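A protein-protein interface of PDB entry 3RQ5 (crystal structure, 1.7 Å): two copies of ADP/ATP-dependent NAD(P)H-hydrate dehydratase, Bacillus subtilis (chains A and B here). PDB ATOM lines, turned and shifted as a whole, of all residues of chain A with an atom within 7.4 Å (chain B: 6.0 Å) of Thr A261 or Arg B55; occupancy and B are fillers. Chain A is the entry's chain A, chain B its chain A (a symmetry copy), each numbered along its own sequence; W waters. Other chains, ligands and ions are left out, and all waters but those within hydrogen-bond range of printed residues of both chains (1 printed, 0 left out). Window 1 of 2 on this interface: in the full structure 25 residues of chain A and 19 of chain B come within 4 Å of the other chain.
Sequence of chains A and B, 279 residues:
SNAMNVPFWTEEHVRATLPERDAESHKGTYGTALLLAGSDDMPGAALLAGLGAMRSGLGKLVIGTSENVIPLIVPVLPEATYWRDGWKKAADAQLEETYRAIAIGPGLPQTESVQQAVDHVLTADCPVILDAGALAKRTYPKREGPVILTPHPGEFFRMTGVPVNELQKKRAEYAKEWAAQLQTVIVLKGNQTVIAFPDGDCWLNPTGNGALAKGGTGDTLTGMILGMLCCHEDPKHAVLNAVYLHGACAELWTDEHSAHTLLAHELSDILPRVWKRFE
The side-chain hydroxyl (OG) of Ser A258 lies close to the backbone NH (N) of His A260 (3.1 Å). NH2 of Arg B21 is in hydrogen-bond range of O of Leu B58 (3.1 Å). The backbone carbonyl oxygen of His A260 lies within hydrogen-bond range of the side-chain amino group of Lys A214, 2.8 Å away. O of Ser A258 is in hydrogen-bond range of OG1 of Thr A261, 2.8 Å away. OE1 of Glu A266 lies within hydrogen-bond range of N of Leu A263, 3.0 Å away. The backbone carbonyl oxygen (O) of Ser A258 is in hydrogen-bond range of the indole nitrogen (NE1) of Trp A253.
Water W1 lies within hydrogen-bond range of O of Glu A256 and O of Arg B273.
Leu B58 touches Lys A214. Arg B55 touches Trp A253 (NH1 to CH2, 3.6 Å). CZ2 of Trp A253 touches CB of Pro B272, 3.6 Å away. O of Pro B272 touches CA of His A257, at 3.3 Å. Arg B273 touches His A257. Trp B275 touches Ser A258. Pro B272 touches Thr A261. Trp B275 touches Thr A261. Met B54 touches Leu A263 (CB to CD2, 3.7 Å). CZ of Arg B55 touches CD1 of Leu A263, at 3.6 Å.
No position is printed for both chains.
Thr A261 touches three residues of chain B. Arg B55 touches just these residues of chain A: Trp A253 (3.6 Å), His A260 (3.6 Å), Thr A261 (2.8 Å), Leu A263 (3.6 Å) and Glu A266 (2.8 Å). Printed residues of chain A within 4 Å of Pro B272: Trp A253, His A257, Ser A258 and Thr A261. Printed residues of chain B within 4 Å of Lys A214: Met B54 and Leu B58. Of the printed residues of chain B, His A257 touches Pro B272 (3.3 Å) and Arg B273 (3.8 Å). Of the printed residues of chain B, Ala A259 touches Arg B21. Ser B268 touches none of the printed residues of chain A. Leu B51 touches none of the printed residues of chain A. The nearest residue of chain A that does not touch Arg B55 is Leu A262 (4.4 Å).
The side-chain carboxylate (OE1) of Glu A256 lies within salt-bridge range of the guanidinium group (NH2) of Arg B273 (2.8 Å). A ring nitrogen (ND1) of His A260 lies within hydrogen-bond range of the guanidinium group (NH1) of Arg B21 (2.9 Å). The guanidinium group (NH2) of Arg B55 lies within salt-bridge range of the side-chain carboxylate (OE2) of Glu A266, 2.8 Å away. NH1 of Arg B55 sits at hydrogen-bond distance from O of Thr A261 (2.8 Å). NZ of Lys A214 lies within hydrogen-bond range of O of Met B54, 2.8 Å away. The backbone NH (N) of Ser A258 sits at hydrogen-bond distance from the backbone carbonyl oxygen (O) of Pro B272, at 2.9 Å. O of His A260 lies within hydrogen-bond range of N of Gly B57 (3.2 Å).
Of the 16 printed residues of chain B, 8 touch a printed residue of chain A. Printed residues of chain B that touch a printed residue of chain A: Arg B21, Met B54, Arg B55, Gly B57, Leu B58, Pro B272, Arg B273 and Trp B275. Hydrophobic or aromatic side chains of chain B within 4 Å of the printed part of chain A: Met B54, Pro B272 and Trp B275. Of the 14 printed residues of chain A, 10 touch a printed residue of chain B. Hydrophobic or aromatic side chains of chain A within 4 Å of the printed part of chain B: Trp A253, His A257, His A260 and Leu A263. Along chain A the printed residues that touch a printed residue of chain B span positions 214 to 266. Among the printed residues, 20 pairs touch across the chains. Among the printed residues, Asp or Glu carboxylates within 4 Å of a Lys or Arg side-chain nitrogen of the other chain: Glu A256 with Arg B273 (2.8 Å) and Glu A266 with Arg B55 (2.8 Å).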
ATOM      1  N   ALA A 211      15.036  16.834 -25.125  1.00  0.00           N
ATOM      2  CA  ALA A 211      16.297  16.091 -25.080  1.00  0.00           C
ATOM      3  C   ALA A 211      16.402  15.150 -26.275  1.00  0.00           C
ATOM      4  O   ALA A 211      17.497  14.740 -26.657  1.00  0.00           O
ATOM      5  CB  ALA A 211      16.441  15.311 -23.794  1.00  0.00           C
ATOM      6  N   LYS A 214      17.864  15.488 -31.105  1.00  0.00           N
ATOM      7  CA  LYS A 214      19.301  15.346 -31.425  1.00  0.00           C
ATOM      8  C   LYS A 214      19.502  14.078 -32.211  1.00  0.00           C
ATOM      9  O   LYS A 214      18.773  13.086 -32.018  1.00  0.00           O
ATOM     10  CB  LYS A 214      20.126  15.320 -30.125  1.00  0.00           C
ATOM     11  CG  LYS A 214      21.638  15.447 -30.344  1.00  0.00           C
ATOM     12  CD  LYS A 214      22.440  15.403 -28.987  1.00  0.00           C
ATOM     13  CE  LYS A 214      22.071  16.561 -28.013  1.00  0.00           C
ATOM     14  NZ  LYS A 214      22.735  16.362 -26.692  1.00  0.00           N
ATOM     15  N   TRP A 253      15.715  11.015 -17.652  1.00  0.00           N
ATOM     16  CA  TRP A 253      16.994  11.711 -17.814  1.00  0.00           C
ATOM     17  C   TRP A 253      16.950  13.126 -17.306  1.00  0.00           C
ATOM     18  O   TRP A 253      17.850  13.543 -16.561  1.00  0.00           O
ATOM     19  CB  TRP A 253      17.410  11.754 -19.307  1.00  0.00           C
ATOM     20  CG  TRP A 253      18.645  12.618 -19.621  1.00  0.00           C
ATOM     21  CD1 TRP A 253      18.658  13.898 -20.122  1.00  0.00           C
ATOM     22  CD2 TRP A 253      20.009  12.228 -19.512  1.00  0.00           C
ATOM     23  NE1 TRP A 253      19.942  14.324 -20.309  1.00  0.00           N
ATOM     24  CE2 TRP A 253      20.795  13.320 -19.943  1.00  0.00           C
ATOM     25  CE3 TRP A 253      20.660  11.068 -19.066  1.00  0.00           C
ATOM     26  CZ2 TRP A 253      22.160  13.266 -19.963  1.00  0.00           C
ATOM     27  CZ3 TRP A 253      22.006  11.013 -19.092  1.00  0.00           C
ATOM     28  CH2 TRP A 253      22.763  12.113 -19.536  1.00  0.00           C
ATOM     29  N   GLU A 256      17.602  14.800 -13.408  1.00  0.00           N
ATOM     30  CA  GLU A 256      18.889  15.175 -12.825  1.00  0.00           C
ATOM     31  C   GLU A 256      19.952  15.655 -13.820  1.00  0.00           C
ATOM     32  O   GLU A 256      21.063  15.999 -13.424  1.00  0.00           O
ATOM     33  CB  GLU A 256      19.436  13.979 -12.078  1.00  0.00           C
ATOM     34  CG  GLU A 256      18.628  13.685 -10.796  1.00  0.00           C
ATOM     35  CD  GLU A 256      19.380  12.741  -9.879  1.00  0.00           C
ATOM     36  OE1 GLU A 256      19.759  11.640 -10.331  1.00  0.00           O
ATOM     37  OE2 GLU A 256      19.605  13.108  -8.716  1.00  0.00           O
ATOM     38  N   HIS A 257      19.586  15.663 -15.086  1.00  0.00           N
ATOM     39  CA  HIS A 257      20.495  16.016 -16.181  1.00  0.00           C
ATOM     40  C   HIS A 257      19.845  17.041 -17.109  1.00  0.00           C
ATOM     41  O   HIS A 257      18.632  16.996 -17.370  1.00  0.00           O
ATOM     42  CB  HIS A 257      20.872  14.791 -16.982  1.00  0.00           C
ATOM     43  CG  HIS A 257      21.289  13.610 -16.167  1.00  0.00           C
ATOM     44  ND1 HIS A 257      20.396  12.657 -15.727  1.00  0.00           N
ATOM     45  CD2 HIS A 257      22.513  13.185 -15.766  1.00  0.00           C
ATOM     46  CE1 HIS A 257      21.042  11.714 -15.061  1.00  0.00           C
ATOM     47  NE2 HIS A 257      22.329  12.012 -15.060  1.00  0.00           N
ATOM     48  N   SER A 258      20.638  17.957 -17.653  1.00  0.00           N
ATOM     49  CA  SER A 258      20.091  18.910 -18.594  1.00  0.00           C
ATOM     50  C   SER A 258      19.591  18.242 -19.868  1.00  0.00           C
ATOM     51  O   SER A 258      20.262  17.382 -20.445  1.00  0.00           O
ATOM     52  CB  SER A 258      21.128  19.979 -18.965  1.00  0.00           C
ATOM     53  OG  SER A 258      20.627  20.766 -20.032  1.00  0.00           O
ATOM     54  N   ALA A 259      18.423  18.688 -20.348  1.00  0.00           N
ATOM     55  CA  ALA A 259      17.891  18.235 -21.612  1.00  0.00           C
ATOM     56  C   ALA A 259      18.791  18.486 -22.800  1.00  0.00           C
ATOM     57  O   ALA A 259      18.670  17.795 -23.837  1.00  0.00           O
ATOM     58  CB  ALA A 259      16.509  18.896 -21.855  1.00  0.00           C
ATOM     59  N   HIS A 260      19.694  19.455 -22.706  1.00  0.00           N
ATOM     60  CA  HIS A 260      20.651  19.688 -23.805  1.00  0.00           C
ATOM     61  C   HIS A 260      21.717  18.634 -23.983  1.00  0.00           C
ATOM     62  O   HIS A 260      22.354  18.600 -25.018  1.00  0.00           O
ATOM     63  CB  HIS A 260      21.389  21.006 -23.595  1.00  0.00           C
ATOM     64  CG  HIS A 260      20.509  22.196 -23.716  1.00  0.00           C
ATOM     65  ND1 HIS A 260      19.949  22.579 -24.917  1.00  0.00           N
ATOM     66  CD2 HIS A 260      20.097  23.099 -22.795  1.00  0.00           C
ATOM     67  CE1 HIS A 260      19.264  23.693 -24.738  1.00  0.00           C
ATOM     68  NE2 HIS A 260      19.317  24.018 -23.454  1.00  0.00           N
ATOM     69  N   THR A 261      21.898  17.765 -23.000  1.00  0.00           N
ATOM     70  CA  THR A 261      23.089  16.939 -22.877  1.00  0.00           C
ATOM     71  C   THR A 261      22.921  15.438 -23.091  1.00  0.00           C
ATOM     72  O   THR A 261      23.898  14.708 -23.030  1.00  0.00           O
ATOM     73  CB  THR A 261      23.736  17.130 -21.511  1.00  0.00           C
ATOM     74  OG1 THR A 261      22.893  16.576 -20.465  1.00  0.00           O
ATOM     75  CG2 THR A 261      23.982  18.637 -21.227  1.00  0.00           C
ATOM     76  N   LEU A 262      21.712  14.989 -23.388  1.00  0.00           N
ATOM     77  CA  LEU A 262      21.437  13.572 -23.601  1.00  0.00           C
ATOM     78  C   LEU A 262      22.092  13.068 -24.870  1.00  0.00           C
ATOM     79  O   LEU A 262      22.044  13.729 -25.889  1.00  0.00           O
ATOM     80  CB  LEU A 262      19.933  13.344 -23.760  1.00  0.00           C
ATOM     81  CG  LEU A 262      19.501  11.877 -24.014  1.00  0.00           C
ATOM     82  CD1 LEU A 262      19.788  10.921 -22.854  1.00  0.00           C
ATOM     83  CD2 LEU A 262      17.972  11.911 -24.352  1.00  0.00           C
ATOM     84  N   LEU A 263      22.663  11.887 -24.788  1.00  0.00           N
ATOM     85  CA  LEU A 263      23.110  11.152 -25.971  1.00  0.00           C
ATOM     86  C   LEU A 263      22.139   9.966 -26.180  1.00  0.00           C
ATOM     87  O   LEU A 263      21.776   9.293 -25.221  1.00  0.00           O
ATOM     88  CB  LEU A 263      24.532  10.676 -25.762  1.00  0.00           C
ATOM     89  CG  LEU A 263      25.591  11.783 -25.585  1.00  0.00           C
ATOM     90  CD1 LEU A 263      26.947  11.187 -25.245  1.00  0.00           C
ATOM     91  CD2 LEU A 263      25.700  12.674 -26.792  1.00  0.00           C
ATOM     92  N   ALA A 264      21.732   9.707 -27.426  1.00  0.00           N
ATOM     93  CA  ALA A 264      20.727   8.712 -27.723  1.00  0.00           C
ATOM     94  C   ALA A 264      20.964   7.370 -27.080  1.00  0.00           C
ATOM     95  O   ALA A 264      20.005   6.744 -26.621  1.00  0.00           O
ATOM     96  CB  ALA A 264      20.643   8.512 -29.253  1.00  0.00           C
ATOM     97  N   HIS A 265      22.199   6.875 -27.105  1.00  0.00           N
ATOM     98  CA  HIS A 265      22.465   5.541 -26.536  1.00  0.00           C
ATOM     99  C   HIS A 265      22.078   5.454 -25.078  1.00  0.00           C
ATOM    100  O   HIS A 265      21.754   4.370 -24.582  1.00  0.00           O
ATOM    101  CB  HIS A 265      23.893   5.084 -26.772  1.00  0.00           C
ATOM    102  CG  HIS A 265      24.909   5.787 -25.936  1.00  0.00           C
ATOM    103  ND1 HIS A 265      25.568   6.912 -26.381  1.00  0.00           N
ATOM    104  CD2 HIS A 265      25.424   5.498 -24.713  1.00  0.00           C
ATOM    105  CE1 HIS A 265      26.432   7.299 -25.452  1.00  0.00           C
ATOM    106  NE2 HIS A 265      26.355   6.470 -24.429  1.00  0.00           N
ATOM    107  N   GLU A 266      22.094   6.584 -24.387  1.00  0.00           N
ATOM    108  CA  GLU A 266      21.696   6.592 -22.996  1.00  0.00           C
ATOM    109  C   GLU A 266      20.222   6.260 -22.776  1.00  0.00           C
ATOM    110  O   GLU A 266      19.842   5.805 -21.679  1.00  0.00           O
ATOM    111  CB  GLU A 266      22.104   7.928 -22.330  1.00  0.00           C
ATOM    112  CG  GLU A 266      23.602   8.058 -22.298  1.00  0.00           C
ATOM    113  CD  GLU A 266      24.078   9.409 -21.843  1.00  0.00           C
ATOM    114  OE1 GLU A 266      23.547  10.448 -22.314  1.00  0.00           O
ATOM    115  OE2 GLU A 266      25.015   9.403 -20.997  1.00  0.00           O
ATOM    116  N   ARG B  21      15.639  24.232 -23.581  1.00  0.00           N
ATOM    117  CA  ARG B  21      15.407  23.315 -24.709  1.00  0.00           C
ATOM    118  C   ARG B  21      13.934  22.986 -24.858  1.00  0.00           C
ATOM    119  O   ARG B  21      13.464  21.981 -24.323  1.00  0.00           O
ATOM    120  CB  ARG B  21      16.215  22.022 -24.581  1.00  0.00           C
ATOM    121  CG  ARG B  21      16.563  21.421 -25.949  1.00  0.00           C
ATOM    122  CD  ARG B  21      17.498  20.244 -25.778  1.00  0.00           C
ATOM    123  NE  ARG B  21      17.941  19.651 -27.047  1.00  0.00           N
ATOM    124  CZ  ARG B  21      18.987  20.041 -27.752  1.00  0.00           C
ATOM    125  NH1 ARG B  21      19.784  21.013 -27.320  1.00  0.00           N
ATOM    126  NH2 ARG B  21      19.271  19.406 -28.881  1.00  0.00           N
ATOM    127  N   GLY B  50      34.378  15.602 -30.034  1.00  0.00           N
ATOM    128  CA  GLY B  50      33.057  15.125 -30.468  1.00  0.00           C
ATOM    129  C   GLY B  50      32.090  14.909 -29.336  1.00  0.00           C
ATOM    130  O   GLY B  50      30.944  15.328 -29.426  1.00  0.00           O
ATOM    131  N   LEU B  51      32.560  14.311 -28.249  1.00  0.00           N
ATOM    132  CA  LEU B  51      31.758  14.079 -27.055  1.00  0.00           C
ATOM    133  C   LEU B  51      31.391  15.422 -26.459  1.00  0.00           C
ATOM    134  O   LEU B  51      30.255  15.641 -26.093  1.00  0.00           O
ATOM    135  CB  LEU B  51      32.572  13.259 -26.060  1.00  0.00           C
ATOM    136  CG  LEU B  51      32.620  11.775 -26.301  1.00  0.00           C
ATOM    137  CD1 LEU B  51      33.866  11.199 -25.510  1.00  0.00           C
ATOM    138  CD2 LEU B  51      31.282  11.100 -25.875  1.00  0.00           C
ATOM    139  N   GLY B  52      32.369  16.330 -26.358  1.00  0.00           N
ATOM    140  CA  GLY B  52      32.072  17.658 -25.797  1.00  0.00           C
ATOM    141  C   GLY B  52      30.996  18.370 -26.589  1.00  0.00           C
ATOM    142  O   GLY B  52      30.112  18.966 -26.027  1.00  0.00           O
ATOM    143  N   ALA B  53      31.059  18.260 -27.922  1.00  0.00           N
ATOM    144  CA  ALA B  53      30.112  18.963 -28.794  1.00  0.00           C
ATOM    145  C   ALA B  53      28.715  18.361 -28.688  1.00  0.00           C
ATOM    146  O   ALA B  53      27.722  19.073 -28.447  1.00  0.00           O
ATOM    147  CB  ALA B  53      30.621  18.920 -30.290  1.00  0.00           C
ATOM    148  N   MET B  54      28.618  17.028 -28.752  1.00  0.00           N
ATOM    149  CA  MET B  54      27.296  16.408 -28.680  1.00  0.00           C
ATOM    150  C   MET B  54      26.654  16.527 -27.324  1.00  0.00           C
ATOM    151  O   MET B  54      25.428  16.567 -27.212  1.00  0.00           O
ATOM    152  CB  MET B  54      27.342  14.943 -29.147  1.00  0.00           C
ATOM    153  CG  MET B  54      27.769  14.862 -30.606  1.00  0.00           C
ATOM    154  SD  MET B  54      27.091  13.437 -31.538  1.00  0.00           S
ATOM    155  CE  MET B  54      25.456  14.027 -31.848  1.00  0.00           C
ATOM    156  N   ARG B  55      27.478  16.594 -26.279  1.00  0.00           N
ATOM    157  CA  ARG B  55      26.975  16.835 -24.946  1.00  0.00           C
ATOM    158  C   ARG B  55      26.461  18.267 -24.766  1.00  0.00           C
ATOM    159  O   ARG B  55      25.770  18.536 -23.782  1.00  0.00           O
ATOM    160  CB  ARG B  55      28.091  16.596 -23.921  1.00  0.00           C
ATOM    161  CG  ARG B  55      28.333  15.156 -23.553  1.00  0.00           C
ATOM    162  CD  ARG B  55      27.248  14.641 -22.694  1.00  0.00           C
ATOM    163  NE  ARG B  55      27.582  13.306 -22.170  1.00  0.00           N
ATOM    164  CZ  ARG B  55      26.687  12.377 -21.834  1.00  0.00           C
ATOM    165  NH1 ARG B  55      25.383  12.569 -21.981  1.00  0.00           N
ATOM    166  NH2 ARG B  55      27.113  11.206 -21.354  1.00  0.00           N
ATOM    167  N   SER B  56      26.814  19.184 -25.662  1.00  0.00           N
ATOM    168  CA  SER B  56      26.597  20.608 -25.426  1.00  0.00           C
ATOM    169  C   SER B  56      25.468  21.249 -26.229  1.00  0.00           C
ATOM    170  O   SER B  56      25.536  22.415 -26.577  1.00  0.00           O
ATOM    171  CB  SER B  56      27.938  21.332 -25.562  1.00  0.00           C
ATOM    172  OG  SER B  56      28.802  20.962 -24.492  1.00  0.00           O
ATOM    173  N   GLY B  57      24.431  20.479 -26.553  1.00  0.00           N
ATOM    174  CA  GLY B  57      23.180  21.061 -27.029  1.00  0.00           C
ATOM    175  C   GLY B  57      22.987  21.285 -28.511  1.00  0.00           C
ATOM    176  O   GLY B  57      22.009  21.919 -28.893  1.00  0.00           O
ATOM    177  N   LEU B  58      23.884  20.765 -29.327  1.00  0.00           N
ATOM    178  CA  LEU B  58      23.678  20.797 -30.757  1.00  0.00           C
ATOM    179  C   LEU B  58      22.530  19.863 -31.173  1.00  0.00           C
ATOM    180  O   LEU B  58      21.960  19.133 -30.330  1.00  0.00           O
ATOM    181  CB  LEU B  58      24.948  20.481 -31.495  1.00  0.00           C
ATOM    182  CG  LEU B  58      25.745  19.220 -31.177  1.00  0.00           C
ATOM    183  CD1 LEU B  58      24.949  17.946 -31.538  1.00  0.00           C
ATOM    184  CD2 LEU B  58      27.084  19.229 -31.911  1.00  0.00           C
ATOM    185  N   SER B 268      32.952  15.654 -19.969  1.00  0.00           N
ATOM    186  CA  SER B 268      31.758  15.476 -20.784  1.00  0.00           C
ATOM    187  C   SER B 268      30.673  14.634 -20.117  1.00  0.00           C
ATOM    188  O   SER B 268      29.510  14.867 -20.318  1.00  0.00           O
ATOM    189  CB  SER B 268      32.115  14.839 -22.127  1.00  0.00           C
ATOM    190  OG  SER B 268      33.000  15.635 -22.796  1.00  0.00           O
ATOM    191  N   ASP B 269      31.101  13.617 -19.388  1.00  0.00           N
ATOM    192  CA  ASP B 269      30.257  12.689 -18.659  1.00  0.00           C
ATOM    193  C   ASP B 269      29.588  13.434 -17.465  1.00  0.00           C
ATOM    194  O   ASP B 269      28.496  13.055 -17.023  1.00  0.00           O
ATOM    195  CB  ASP B 269      31.027  11.501 -17.981  1.00  0.00           C
ATOM    196  CG  ASP B 269      31.708  10.469 -18.923  1.00  0.00           C
ATOM    197  OD1 ASP B 269      31.364  10.297 -20.094  1.00  0.00           O
ATOM    198  OD2 ASP B 269      32.609   9.720 -18.384  1.00  0.00           O
ATOM    199  N   LEU B 271      29.136  16.889 -17.274  1.00  0.00           N
ATOM    200  CA  LEU B 271      28.413  18.055 -17.765  1.00  0.00           C
ATOM    201  C   LEU B 271      26.886  17.925 -17.640  1.00  0.00           C
ATOM    202  O   LEU B 271      26.240  18.903 -17.281  1.00  0.00           O
ATOM    203  CB  LEU B 271      28.852  18.423 -19.191  1.00  0.00           C
ATOM    204  CG  LEU B 271      28.192  19.654 -19.814  1.00  0.00           C
ATOM    205  CD1 LEU B 271      28.527  20.948 -19.022  1.00  0.00           C
ATOM    206  CD2 LEU B 271      28.551  19.789 -21.296  1.00  0.00           C
ATOM    207  N   PRO B 272      26.308  16.742 -17.931  1.00  0.00           N
ATOM    208  CA  PRO B 272      24.827  16.664 -17.796  1.00  0.00           C
ATOM    209  C   PRO B 272      24.283  17.099 -16.443  1.00  0.00           C
ATOM    210  O   PRO B 272      23.288  17.812 -16.381  1.00  0.00           O
ATOM    211  CB  PRO B 272      24.534  15.192 -18.025  1.00  0.00           C
ATOM    212  CG  PRO B 272      25.632  14.800 -19.074  1.00  0.00           C
ATOM    213  CD  PRO B 272      26.864  15.562 -18.616  1.00  0.00           C
ATOM    214  N   ARG B 273      24.936  16.651 -15.393  1.00  0.00           N
ATOM    215  CA  ARG B 273      24.514  16.971 -14.023  1.00  0.00           C
ATOM    216  C   ARG B 273      24.862  18.398 -13.661  1.00  0.00           C
ATOM    217  O   ARG B 273      24.073  19.089 -12.997  1.00  0.00           O
ATOM    218  CB  ARG B 273      25.225  16.040 -13.018  1.00  0.00           C
ATOM    219  CG  ARG B 273      24.755  14.660 -13.099  1.00  0.00           C
ATOM    220  CD  ARG B 273      25.349  13.767 -11.993  1.00  0.00           C
ATOM    221  NE  ARG B 273      24.371  12.719 -11.754  1.00  0.00           N
ATOM    222  CZ  ARG B 273      23.274  12.848 -11.013  1.00  0.00           C
ATOM    223  NH1 ARG B 273      23.001  13.969 -10.360  1.00  0.00           N
ATOM    224  NH2 ARG B 273      22.446  11.836 -10.932  1.00  0.00           N
ATOM    225  N   TRP B 275      25.282  21.037 -15.722  1.00  0.00           N
ATOM    226  CA  TRP B 275      24.405  21.950 -16.466  1.00  0.00           C
ATOM    227  C   TRP B 275      23.018  22.037 -15.795  1.00  0.00           C
ATOM    228  O   TRP B 275      22.481  23.135 -15.653  1.00  0.00           O
ATOM    229  CB  TRP B 275      24.354  21.520 -17.937  1.00  0.00           C
ATOM    230  CG  TRP B 275      23.719  22.463 -18.908  1.00  0.00           C
ATOM    231  CD1 TRP B 275      22.661  23.314 -18.722  1.00  0.00           C
ATOM    232  CD2 TRP B 275      24.104  22.594 -20.274  1.00  0.00           C
ATOM    233  NE1 TRP B 275      22.366  23.954 -19.903  1.00  0.00           N
ATOM    234  CE2 TRP B 275      23.233  23.532 -20.868  1.00  0.00           C
ATOM    235  CE3 TRP B 275      25.081  21.992 -21.051  1.00  0.00           C
ATOM    236  CZ2 TRP B 275      23.314  23.882 -22.216  1.00  0.00           C
ATOM    237  CZ3 TRP B 275      25.177  22.347 -22.397  1.00  0.00           C
ATOM    238  CH2 TRP B 275      24.302  23.316 -22.954  1.00  0.00           C
HETATM  239  O   HOH W   1      21.907  17.647 -11.271  1.00  0.00           O
